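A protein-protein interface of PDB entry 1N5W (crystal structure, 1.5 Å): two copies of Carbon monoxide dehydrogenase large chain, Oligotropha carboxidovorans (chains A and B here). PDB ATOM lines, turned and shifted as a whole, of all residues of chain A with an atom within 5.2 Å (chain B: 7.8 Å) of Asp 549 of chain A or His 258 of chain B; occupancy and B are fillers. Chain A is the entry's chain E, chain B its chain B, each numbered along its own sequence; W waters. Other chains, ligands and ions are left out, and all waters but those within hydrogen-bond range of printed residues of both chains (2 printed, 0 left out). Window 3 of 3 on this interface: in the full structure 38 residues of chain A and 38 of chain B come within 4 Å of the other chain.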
ATOM      1  N   LYS A  17      -4.166  25.411 -20.659  1.00  0.00           N
ATOM      2  CA  LYS A  17      -3.415  24.424 -21.395  1.00  0.00           C
ATOM      3  C   LYS A  17      -3.835  22.988 -20.996  1.00  0.00           C
ATOM      4  O   LYS A  17      -3.590  22.052 -21.748  1.00  0.00           O
ATOM      5  CB  LYS A  17      -1.888  24.647 -21.211  1.00  0.00           C
ATOM      6  N   GLN A  19      -6.752  21.015 -20.430  1.00  0.00           N
ATOM      7  CA  GLN A  19      -7.720  20.274 -21.272  1.00  0.00           C
ATOM      8  C   GLN A  19      -7.972  18.863 -20.830  1.00  0.00           C
ATOM      9  O   GLN A  19      -7.925  17.876 -21.631  1.00  0.00           O
ATOM     10  CB  GLN A  19      -7.307  20.345 -22.736  1.00  0.00           C
ATOM     11  CG  GLN A  19      -7.160  21.758 -23.159  1.00  0.00           C
ATOM     12  CD  GLN A  19      -7.259  21.904 -24.596  1.00  0.00           C
ATOM     13  OE1 GLN A  19      -8.350  21.840 -25.145  1.00  0.00           O
ATOM     14  NE2 GLN A  19      -6.098  21.927 -25.261  1.00  0.00           N
ATOM     15  N   ARG A  25     -12.653  19.167 -25.219  1.00  0.00           N
ATOM     16  CA  ARG A  25     -11.415  19.250 -25.959  1.00  0.00           C
ATOM     17  C   ARG A  25     -11.603  18.918 -27.431  1.00  0.00           C
ATOM     18  O   ARG A  25     -12.194  17.875 -27.733  1.00  0.00           O
ATOM     19  CB  ARG A  25     -10.384  18.307 -25.365  1.00  0.00           C
ATOM     20  CG  ARG A  25      -9.044  18.338 -26.052  1.00  0.00           C
ATOM     21  CD  ARG A  25      -8.012  17.353 -25.491  1.00  0.00           C
ATOM     22  NE  ARG A  25      -6.723  17.543 -26.186  1.00  0.00           N
ATOM     23  CZ  ARG A  25      -5.828  16.594 -26.470  1.00  0.00           C
ATOM     24  NH1 ARG A  25      -6.017  15.301 -26.210  1.00  0.00           N
ATOM     25  NH2 ARG A  25      -4.642  16.927 -26.993  1.00  0.00           N
ATOM     26  N   VAL A  28      -7.730  15.814 -31.746  1.00  0.00           N
ATOM     27  CA  VAL A  28      -6.436  15.820 -32.410  1.00  0.00           C
ATOM     28  C   VAL A  28      -6.492  15.121 -33.768  1.00  0.00           C
ATOM     29  O   VAL A  28      -5.755  15.511 -34.694  1.00  0.00           O
ATOM     30  CB  VAL A  28      -5.318  15.233 -31.556  1.00  0.00           C
ATOM     31  CG1 VAL A  28      -5.017  16.158 -30.358  1.00  0.00           C
ATOM     32  CG2 VAL A  28      -5.601  13.807 -31.085  1.00  0.00           C
ATOM     33  N   HIS A 514       8.674  11.358 -20.605  1.00  0.00           N
ATOM     34  CA  HIS A 514      10.009  11.657 -21.114  1.00  0.00           C
ATOM     35  C   HIS A 514      10.738  12.641 -20.186  1.00  0.00           C
ATOM     36  O   HIS A 514      10.103  13.247 -19.296  1.00  0.00           O
ATOM     37  CB  HIS A 514       9.868  12.292 -22.497  1.00  0.00           C
ATOM     38  CG  HIS A 514       9.285  11.370 -23.510  1.00  0.00           C
ATOM     39  ND1 HIS A 514       9.564  10.008 -23.553  1.00  0.00           N
ATOM     40  CD2 HIS A 514       8.461  11.616 -24.562  1.00  0.00           C
ATOM     41  CE1 HIS A 514       8.870   9.474 -24.557  1.00  0.00           C
ATOM     42  NE2 HIS A 514       8.235  10.431 -25.211  1.00  0.00           N
ATOM     43  N   SER A 518       6.885  15.514 -21.560  1.00  0.00           N
ATOM     44  CA  SER A 518       5.862  15.047 -22.466  1.00  0.00           C
ATOM     45  C   SER A 518       5.794  13.521 -22.397  1.00  0.00           C
ATOM     46  O   SER A 518       6.533  12.911 -21.594  1.00  0.00           O
ATOM     47  CB  SER A 518       6.196  15.502 -23.903  1.00  0.00           C
ATOM     48  OG  SER A 518       7.492  15.040 -24.287  1.00  0.00           O
ATOM     49  N   VAL A 519       4.773  12.952 -23.011  1.00  0.00           N
ATOM     50  CA  VAL A 519       4.296  11.611 -22.697  1.00  0.00           C
ATOM     51  C   VAL A 519       3.949  10.840 -23.982  1.00  0.00           C
ATOM     52  O   VAL A 519       3.327  11.403 -24.900  1.00  0.00           O
ATOM     53  CB  VAL A 519       3.021  11.700 -21.828  1.00  0.00           C
ATOM     54  CG1 VAL A 519       2.543  10.306 -21.467  1.00  0.00           C
ATOM     55  CG2 VAL A 519       3.236  12.565 -20.609  1.00  0.00           C
ATOM     56  N   ILE A 520       4.329   9.554 -24.015  1.00  0.00           N
ATOM     57  CA  ILE A 520       3.773   8.601 -24.984  1.00  0.00           C
ATOM     58  C   ILE A 520       2.954   7.553 -24.235  1.00  0.00           C
ATOM     59  O   ILE A 520       3.448   6.969 -23.241  1.00  0.00           O
ATOM     60  CB  ILE A 520       4.840   7.924 -25.906  1.00  0.00           C
ATOM     61  CG1 ILE A 520       4.256   6.865 -26.800  1.00  0.00           C
ATOM     62  CG2 ILE A 520       5.981   7.298 -25.123  1.00  0.00           C
ATOM     63  CD1 ILE A 520       3.278   7.374 -27.850  1.00  0.00           C
ATOM     64  N   PRO A 547      -0.422  18.889 -19.466  1.00  0.00           N
ATOM     65  CA  PRO A 547      -1.367  19.325 -20.494  1.00  0.00           C
ATOM     66  C   PRO A 547      -1.660  18.207 -21.492  1.00  0.00           C
ATOM     67  O   PRO A 547      -0.742  17.458 -21.906  1.00  0.00           O
ATOM     68  CB  PRO A 547      -0.590  20.455 -21.170  1.00  0.00           C
ATOM     69  CG  PRO A 547       0.285  20.984 -20.103  1.00  0.00           C
ATOM     70  CD  PRO A 547       0.681  19.840 -19.274  1.00  0.00           C
ATOM     71  N   ALA A 548      -2.902  18.084 -21.932  1.00  0.00           N
ATOM     72  CA  ALA A 548      -3.269  17.044 -22.866  1.00  0.00           C
ATOM     73  C   ALA A 548      -2.487  17.060 -24.173  1.00  0.00           C
ATOM     74  O   ALA A 548      -2.181  15.990 -24.722  1.00  0.00           O
ATOM     75  CB  ALA A 548      -4.806  17.032 -23.172  1.00  0.00           C
ATOM     76  N   ASP A 549      -2.088  18.222 -24.643  1.00  0.00           N
ATOM     77  CA  ASP A 549      -1.346  18.310 -25.900  1.00  0.00           C
ATOM     78  C   ASP A 549       0.085  17.872 -25.742  1.00  0.00           C
ATOM     79  O   ASP A 549       0.749  17.638 -26.759  1.00  0.00           O
ATOM     80  CB  ASP A 549      -1.379  19.673 -26.518  1.00  0.00           C
ATOM     81  CG  ASP A 549      -2.673  19.948 -27.181  1.00  0.00           C
ATOM     82  OD1 ASP A 549      -3.113  19.150 -28.103  1.00  0.00           O
ATOM     83  OD2 ASP A 549      -3.203  21.025 -26.867  1.00  0.00           O
ATOM     84  N   ASP A 550       0.529  17.643 -24.486  1.00  0.00           N
ATOM     85  CA  ASP A 550       1.867  17.136 -24.212  1.00  0.00           C
ATOM     86  C   ASP A 550       1.859  15.596 -24.132  1.00  0.00           C
ATOM     87  O   ASP A 550       2.887  15.018 -23.813  1.00  0.00           O
ATOM     88  CB  ASP A 550       2.447  17.634 -22.884  1.00  0.00           C
ATOM     89  CG  ASP A 550       2.690  19.114 -22.829  1.00  0.00           C
ATOM     90  OD1 ASP A 550       2.604  19.762 -23.885  1.00  0.00           O
ATOM     91  OD2 ASP A 550       3.048  19.679 -21.775  1.00  0.00           O
ATOM     92  N   ILE A 551       0.754  14.981 -24.536  1.00  0.00           N
ATOM     93  CA  ILE A 551       0.577  13.535 -24.468  1.00  0.00           C
ATOM     94  C   ILE A 551       0.184  13.004 -25.832  1.00  0.00           C
ATOM     95  O   ILE A 551      -0.786  13.476 -26.417  1.00  0.00           O
ATOM     96  CB  ILE A 551      -0.550  13.203 -23.439  1.00  0.00           C
ATOM     97  CG1 ILE A 551      -0.179  13.766 -22.029  1.00  0.00           C
ATOM     98  CG2 ILE A 551      -0.770  11.677 -23.353  1.00  0.00           C
ATOM     99  CD1 ILE A 551      -1.331  13.849 -21.060  1.00  0.00           C
ATOM    100  N   MET A 552       0.885  11.985 -26.276  1.00  0.00           N
ATOM    101  CA  MET A 552       0.614  11.288 -27.553  1.00  0.00           C
ATOM    102  C   MET A 552      -0.085   9.993 -27.243  1.00  0.00           C
ATOM    103  O   MET A 552       0.443   9.225 -26.487  1.00  0.00           O
ATOM    104  CB  MET A 552       1.908  11.012 -28.301  1.00  0.00           C
ATOM    105  CG  MET A 552       1.715  10.301 -29.629  1.00  0.00           C
ATOM    106  SD  MET A 552       0.794  11.266 -30.841  1.00  0.00           S
ATOM    107  CE  MET A 552       1.850  12.660 -31.190  1.00  0.00           C
ATOM    108  N   GLY B 231       2.855  18.672 -37.297  1.00  0.00           N
ATOM    109  CA  GLY B 231       3.794  19.243 -36.353  1.00  0.00           C
ATOM    110  C   GLY B 231       4.718  18.219 -35.706  1.00  0.00           C
ATOM    111  O   GLY B 231       5.098  18.349 -34.525  1.00  0.00           O
ATOM    112  N   GLU B 232       5.085  17.180 -36.442  1.00  0.00           N
ATOM    113  CA  GLU B 232       5.952  16.140 -35.900  1.00  0.00           C
ATOM    114  C   GLU B 232       7.142  15.858 -36.777  1.00  0.00           C
ATOM    115  O   GLU B 232       7.017  15.767 -37.991  1.00  0.00           O
ATOM    116  CB  GLU B 232       5.169  14.801 -35.779  1.00  0.00           C
ATOM    117  CG  GLU B 232       3.965  14.878 -34.846  1.00  0.00           C
ATOM    118  CD  GLU B 232       3.123  13.630 -34.793  1.00  0.00           C
ATOM    119  OE1 GLU B 232       3.653  12.516 -34.982  1.00  0.00           O
ATOM    120  OE2 GLU B 232       1.906  13.777 -34.513  1.00  0.00           O
ATOM    121  N   LEU B 233       8.316  15.734 -36.144  1.00  0.00           N
ATOM    122  CA  LEU B 233       9.548  15.504 -36.839  1.00  0.00           C
ATOM    123  C   LEU B 233       9.930  14.023 -36.741  1.00  0.00           C
ATOM    124  O   LEU B 233       9.974  13.493 -35.618  1.00  0.00           O
ATOM    125  CB  LEU B 233      10.680  16.324 -36.186  1.00  0.00           C
ATOM    126  CG  LEU B 233      12.108  16.080 -36.716  1.00  0.00           C
ATOM    127  CD1 LEU B 233      12.186  16.542 -38.133  1.00  0.00           C
ATOM    128  CD2 LEU B 233      13.153  16.784 -35.841  1.00  0.00           C
ATOM    129  N   ARG B 246      17.278  12.549 -29.417  1.00  0.00           N
ATOM    130  CA  ARG B 246      15.934  13.079 -29.283  1.00  0.00           C
ATOM    131  C   ARG B 246      15.918  14.245 -28.297  1.00  0.00           C
ATOM    132  O   ARG B 246      15.312  15.296 -28.570  1.00  0.00           O
ATOM    133  CB  ARG B 246      14.884  12.023 -28.912  1.00  0.00           C
ATOM    134  CG  ARG B 246      13.499  12.549 -28.996  1.00  0.00           C
ATOM    135  CD  ARG B 246      12.450  11.615 -28.427  1.00  0.00           C
ATOM    136  NE  ARG B 246      12.583  11.439 -26.980  1.00  0.00           N
ATOM    137  CZ  ARG B 246      12.131  10.440 -26.274  1.00  0.00           C
ATOM    138  NH1 ARG B 246      11.502   9.414 -26.834  1.00  0.00           N
ATOM    139  NH2 ARG B 246      12.399  10.444 -24.981  1.00  0.00           N
ATOM    140  N   SER B 250      15.092  18.123 -29.136  1.00  0.00           N
ATOM    141  CA  SER B 250      14.003  18.842 -28.477  1.00  0.00           C
ATOM    142  C   SER B 250      14.498  20.171 -27.879  1.00  0.00           C
ATOM    143  O   SER B 250      13.889  21.216 -28.039  1.00  0.00           O
ATOM    144  CB  SER B 250      13.403  17.945 -27.379  1.00  0.00           C
ATOM    145  OG  SER B 250      12.313  18.601 -26.733  1.00  0.00           O
ATOM    146  N   LEU B 255      10.681  21.642 -30.290  1.00  0.00           N
ATOM    147  CA  LEU B 255       9.622  20.634 -30.456  1.00  0.00           C
ATOM    148  C   LEU B 255       9.663  19.735 -29.252  1.00  0.00           C
ATOM    149  O   LEU B 255      10.769  19.408 -28.804  1.00  0.00           O
ATOM    150  CB  LEU B 255       9.843  19.809 -31.733  1.00  0.00           C
ATOM    151  CG  LEU B 255       9.719  20.535 -33.072  1.00  0.00           C
ATOM    152  CD1 LEU B 255      10.241  19.630 -34.184  1.00  0.00           C
ATOM    153  CD2 LEU B 255       8.255  20.904 -33.253  1.00  0.00           C
ATOM    154  N   PRO B 256       8.522  19.260 -28.758  1.00  0.00           N
ATOM    155  CA  PRO B 256       8.476  18.415 -27.575  1.00  0.00           C
ATOM    156  C   PRO B 256       8.843  16.978 -27.967  1.00  0.00           C
ATOM    157  O   PRO B 256       8.631  16.560 -29.111  1.00  0.00           O
ATOM    158  CB  PRO B 256       7.030  18.540 -27.121  1.00  0.00           C
ATOM    159  CG  PRO B 256       6.239  18.770 -28.408  1.00  0.00           C
ATOM    160  CD  PRO B 256       7.176  19.623 -29.259  1.00  0.00           C
ATOM    161  N   GLU B 257       9.345  16.222 -26.990  1.00  0.00           N
ATOM    162  CA  GLU B 257       9.855  14.903 -27.261  1.00  0.00           C
ATOM    163  C   GLU B 257       8.840  13.918 -27.822  1.00  0.00           C
ATOM    164  O   GLU B 257       9.253  13.032 -28.620  1.00  0.00           O
ATOM    165  CB  GLU B 257      10.559  14.331 -26.046  1.00  0.00           C
ATOM    166  CG  GLU B 257      11.849  15.023 -25.670  1.00  0.00           C
ATOM    167  CD  GLU B 257      12.598  14.310 -24.537  1.00  0.00           C
ATOM    168  OE1 GLU B 257      13.266  13.281 -24.839  1.00  0.00           O
ATOM    169  OE2 GLU B 257      12.465  14.697 -23.352  1.00  0.00           O
ATOM    170  N   HIS B 258       7.576  14.012 -27.443  1.00  0.00           N
ATOM    171  CA  HIS B 258       6.549  13.108 -27.968  1.00  0.00           C
ATOM    172  C   HIS B 258       6.275  13.344 -29.451  1.00  0.00           C
ATOM    173  O   HIS B 258       5.518  12.561 -30.056  1.00  0.00           O
ATOM    174  CB  HIS B 258       5.250  13.137 -27.127  1.00  0.00           C
ATOM    175  CG  HIS B 258       4.541  14.436 -27.140  1.00  0.00           C
ATOM    176  ND1 HIS B 258       3.169  14.610 -27.277  1.00  0.00           N
ATOM    177  CD2 HIS B 258       5.056  15.671 -26.993  1.00  0.00           C
ATOM    178  CE1 HIS B 258       2.898  15.920 -27.259  1.00  0.00           C
ATOM    179  NE2 HIS B 258       4.031  16.565 -27.068  1.00  0.00           N
ATOM    180  N   LYS B 259       6.704  14.496 -29.968  1.00  0.00           N
ATOM    181  CA  LYS B 259       6.537  14.819 -31.375  1.00  0.00           C
ATOM    182  C   LYS B 259       7.845  14.748 -32.165  1.00  0.00           C
ATOM    183  O   LYS B 259       7.890  15.285 -33.277  1.00  0.00           O
ATOM    184  CB  LYS B 259       5.759  16.128 -31.541  1.00  0.00           C
ATOM    185  CG  LYS B 259       4.359  16.045 -30.982  1.00  0.00           C
ATOM    186  CD  LYS B 259       3.533  17.250 -31.118  1.00  0.00           C
ATOM    187  CE  LYS B 259       2.106  17.007 -30.645  1.00  0.00           C
ATOM    188  NZ  LYS B 259       1.285  18.223 -30.770  1.00  0.00           N
ATOM    189  N   ILE B 260       8.873  14.096 -31.597  1.00  0.00           N
ATOM    190  CA  ILE B 260      10.141  13.850 -32.306  1.00  0.00           C
ATOM    191  C   ILE B 260      10.378  12.346 -32.288  1.00  0.00           C
ATOM    192  O   ILE B 260      10.565  11.775 -31.237  1.00  0.00           O
ATOM    193  CB  ILE B 260      11.346  14.566 -31.622  1.00  0.00           C
ATOM    194  CG1 ILE B 260      11.130  16.085 -31.522  1.00  0.00           C
ATOM    195  CG2 ILE B 260      12.618  14.242 -32.348  1.00  0.00           C
ATOM    196  CD1 ILE B 260      12.179  16.796 -30.707  1.00  0.00           C
ATOM    197  N   HIS B 261      10.338  11.722 -33.467  1.00  0.00           N
ATOM    198  CA  HIS B 261      10.422  10.298 -33.640  1.00  0.00           C
ATOM    199  C   HIS B 261      11.796   9.994 -34.205  1.00  0.00           C
ATOM    200  O   HIS B 261      11.997  10.112 -35.417  1.00  0.00           O
ATOM    201  CB  HIS B 261       9.311   9.827 -34.581  1.00  0.00           C
ATOM    202  CG  HIS B 261       7.965  10.385 -34.248  1.00  0.00           C
ATOM    203  ND1 HIS B 261       7.389  10.248 -32.994  1.00  0.00           N
ATOM    204  CD2 HIS B 261       7.124  11.152 -34.981  1.00  0.00           C
ATOM    205  CE1 HIS B 261       6.241  10.909 -32.991  1.00  0.00           C
ATOM    206  NE2 HIS B 261       6.042  11.448 -34.188  1.00  0.00           N
ATOM    207  N   ASP B 559      10.320   6.154 -30.061  1.00  0.00           N
ATOM    208  CA  ASP B 559       8.903   6.029 -29.700  1.00  0.00           C
ATOM    209  C   ASP B 559       8.599   4.739 -28.923  1.00  0.00           C
ATOM    210  O   ASP B 559       7.668   4.685 -28.129  1.00  0.00           O
ATOM    211  CB  ASP B 559       8.022   5.974 -30.943  1.00  0.00           C
ATOM    212  CG  ASP B 559       7.792   7.313 -31.640  1.00  0.00           C
ATOM    213  OD1 ASP B 559       8.222   8.417 -31.253  1.00  0.00           O
ATOM    214  OD2 ASP B 559       7.146   7.298 -32.737  1.00  0.00           O
HETATM  215  O   HOH W   1       8.953  17.333 -24.308  1.00  0.00           O
HETATM  216  O   HOH W   2      -1.178  17.386 -29.578  1.00  0.00           O
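Among the printed residues, pairs that only touch across the chains: Val 519 of chain A with His 258 of chain B, Met 552 of chain A with Glu 232 of chain B, Ile 551 of chain A with His 258 of chain B, Met 552 of chain A with His 258 of chain B, His 514 of chain A with Glu 257 of chain B and His 514 of chain A with His 258 of chain B.
No position is printed for both chains.
Of the 11 pairs that touch across the chains among the printed residues, none has its exchanged pair printed and touching as well.
The side-chain carboxylate of Glu 232 of chain B is in hydrogen-bond range of a ring nitrogen (NE2) of His 261 of chain B, 2.7 Å away.
The guanidinium group (NE) of Arg 246 of chain B is in salt-bridge range of the side-chain carboxylate (OE1) of Glu 257 of chain B (2.9 Å).
NE2 of Gln 19 of chain A sits at hydrogen-bond distance from OD2 of Asp 549 of chain A, at 3.4 Å.
NH2 of Arg 25 of chain A is in salt-bridge range of OD1 of Asp 549 of chain A.
N of Val 519 of chain A lies within hydrogen-bond range of O of Asp 550 of chain A (2.9 Å).
N of Met 552 of chain A sits at hydrogen-bond distance from O of Val 519 of chain A.
Pro 547 of chain A touches none of the printed residues of chain B.
No residue of chain B comes within 4 Å of Ala 548 of chain A.
Of chain B, only His 258 (2.8 Å) comes within 4 Å of Asp 549 of chain A.
Of the printed residues of chain B, Asp 550 of chain A touches His 258 (3.3 Å).
Of the printed residues of chain B, Ile 551 of chain A touches His 258.
Ser 250 of chain B touches none of the printed residues of chain A.
Of chain A, only His 514 (3.9 Å), Ser 518 (3.3 Å), Val 519 (3.4 Å), Asp 549 (2.8 Å), Asp 550 (3.3 Å), Ile 551 (3.6 Å) and Met 552 (3.6 Å) come within 4 Å of His 258 of chain B.
The nearest residue of chain A that does not touch His 258 of chain B is Ile 520 of chain A (4.8 Å).
The nearest printed residue of chain B that does not touch Val 519 of chain A is Glu 257 of chain B (6.4 Å).
The guanidinium group (NH2) of Arg 246 of chain B is in hydrogen-bond range of a ring nitrogen (ND1) of His 514 of chain A, at 3.2 Å.
N of Glu 257 of chain B lies within hydrogen-bond range of OG of Ser 518 of chain A (3.5 Å).
The backbone NH of His 258 of chain B lies within hydrogen-bond range of the side-chain hydroxyl of Ser 518 of chain A, at 3.3 Å.
The backbone carbonyl oxygen of Asp 549 of chain A sits close to a ring nitrogen (NE2) of His 258 of chain B (3.5 Å).
ND1 of His 258 of chain B sits at hydrogen-bond distance from O of Asp 550 of chain A, at 3.5 Å.
Of the 14 printed residues of chain A, 7 touch a printed residue of chain B.
Hydrophobic or aromatic side chains of chain B that line the printed part of chain A: His 258.
Water W1 bridges OG of Ser 518 of chain A (2.7 Å) and N of Glu 257 of chain B (2.9 Å).
Water W2 lies within hydrogen-bond range of the side-chain amino group (NZ) of Lys 259 of chain B (2.9 Å) and the side-chain carboxylate (OD1) of Asp 549 of chain A (3.0 Å).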
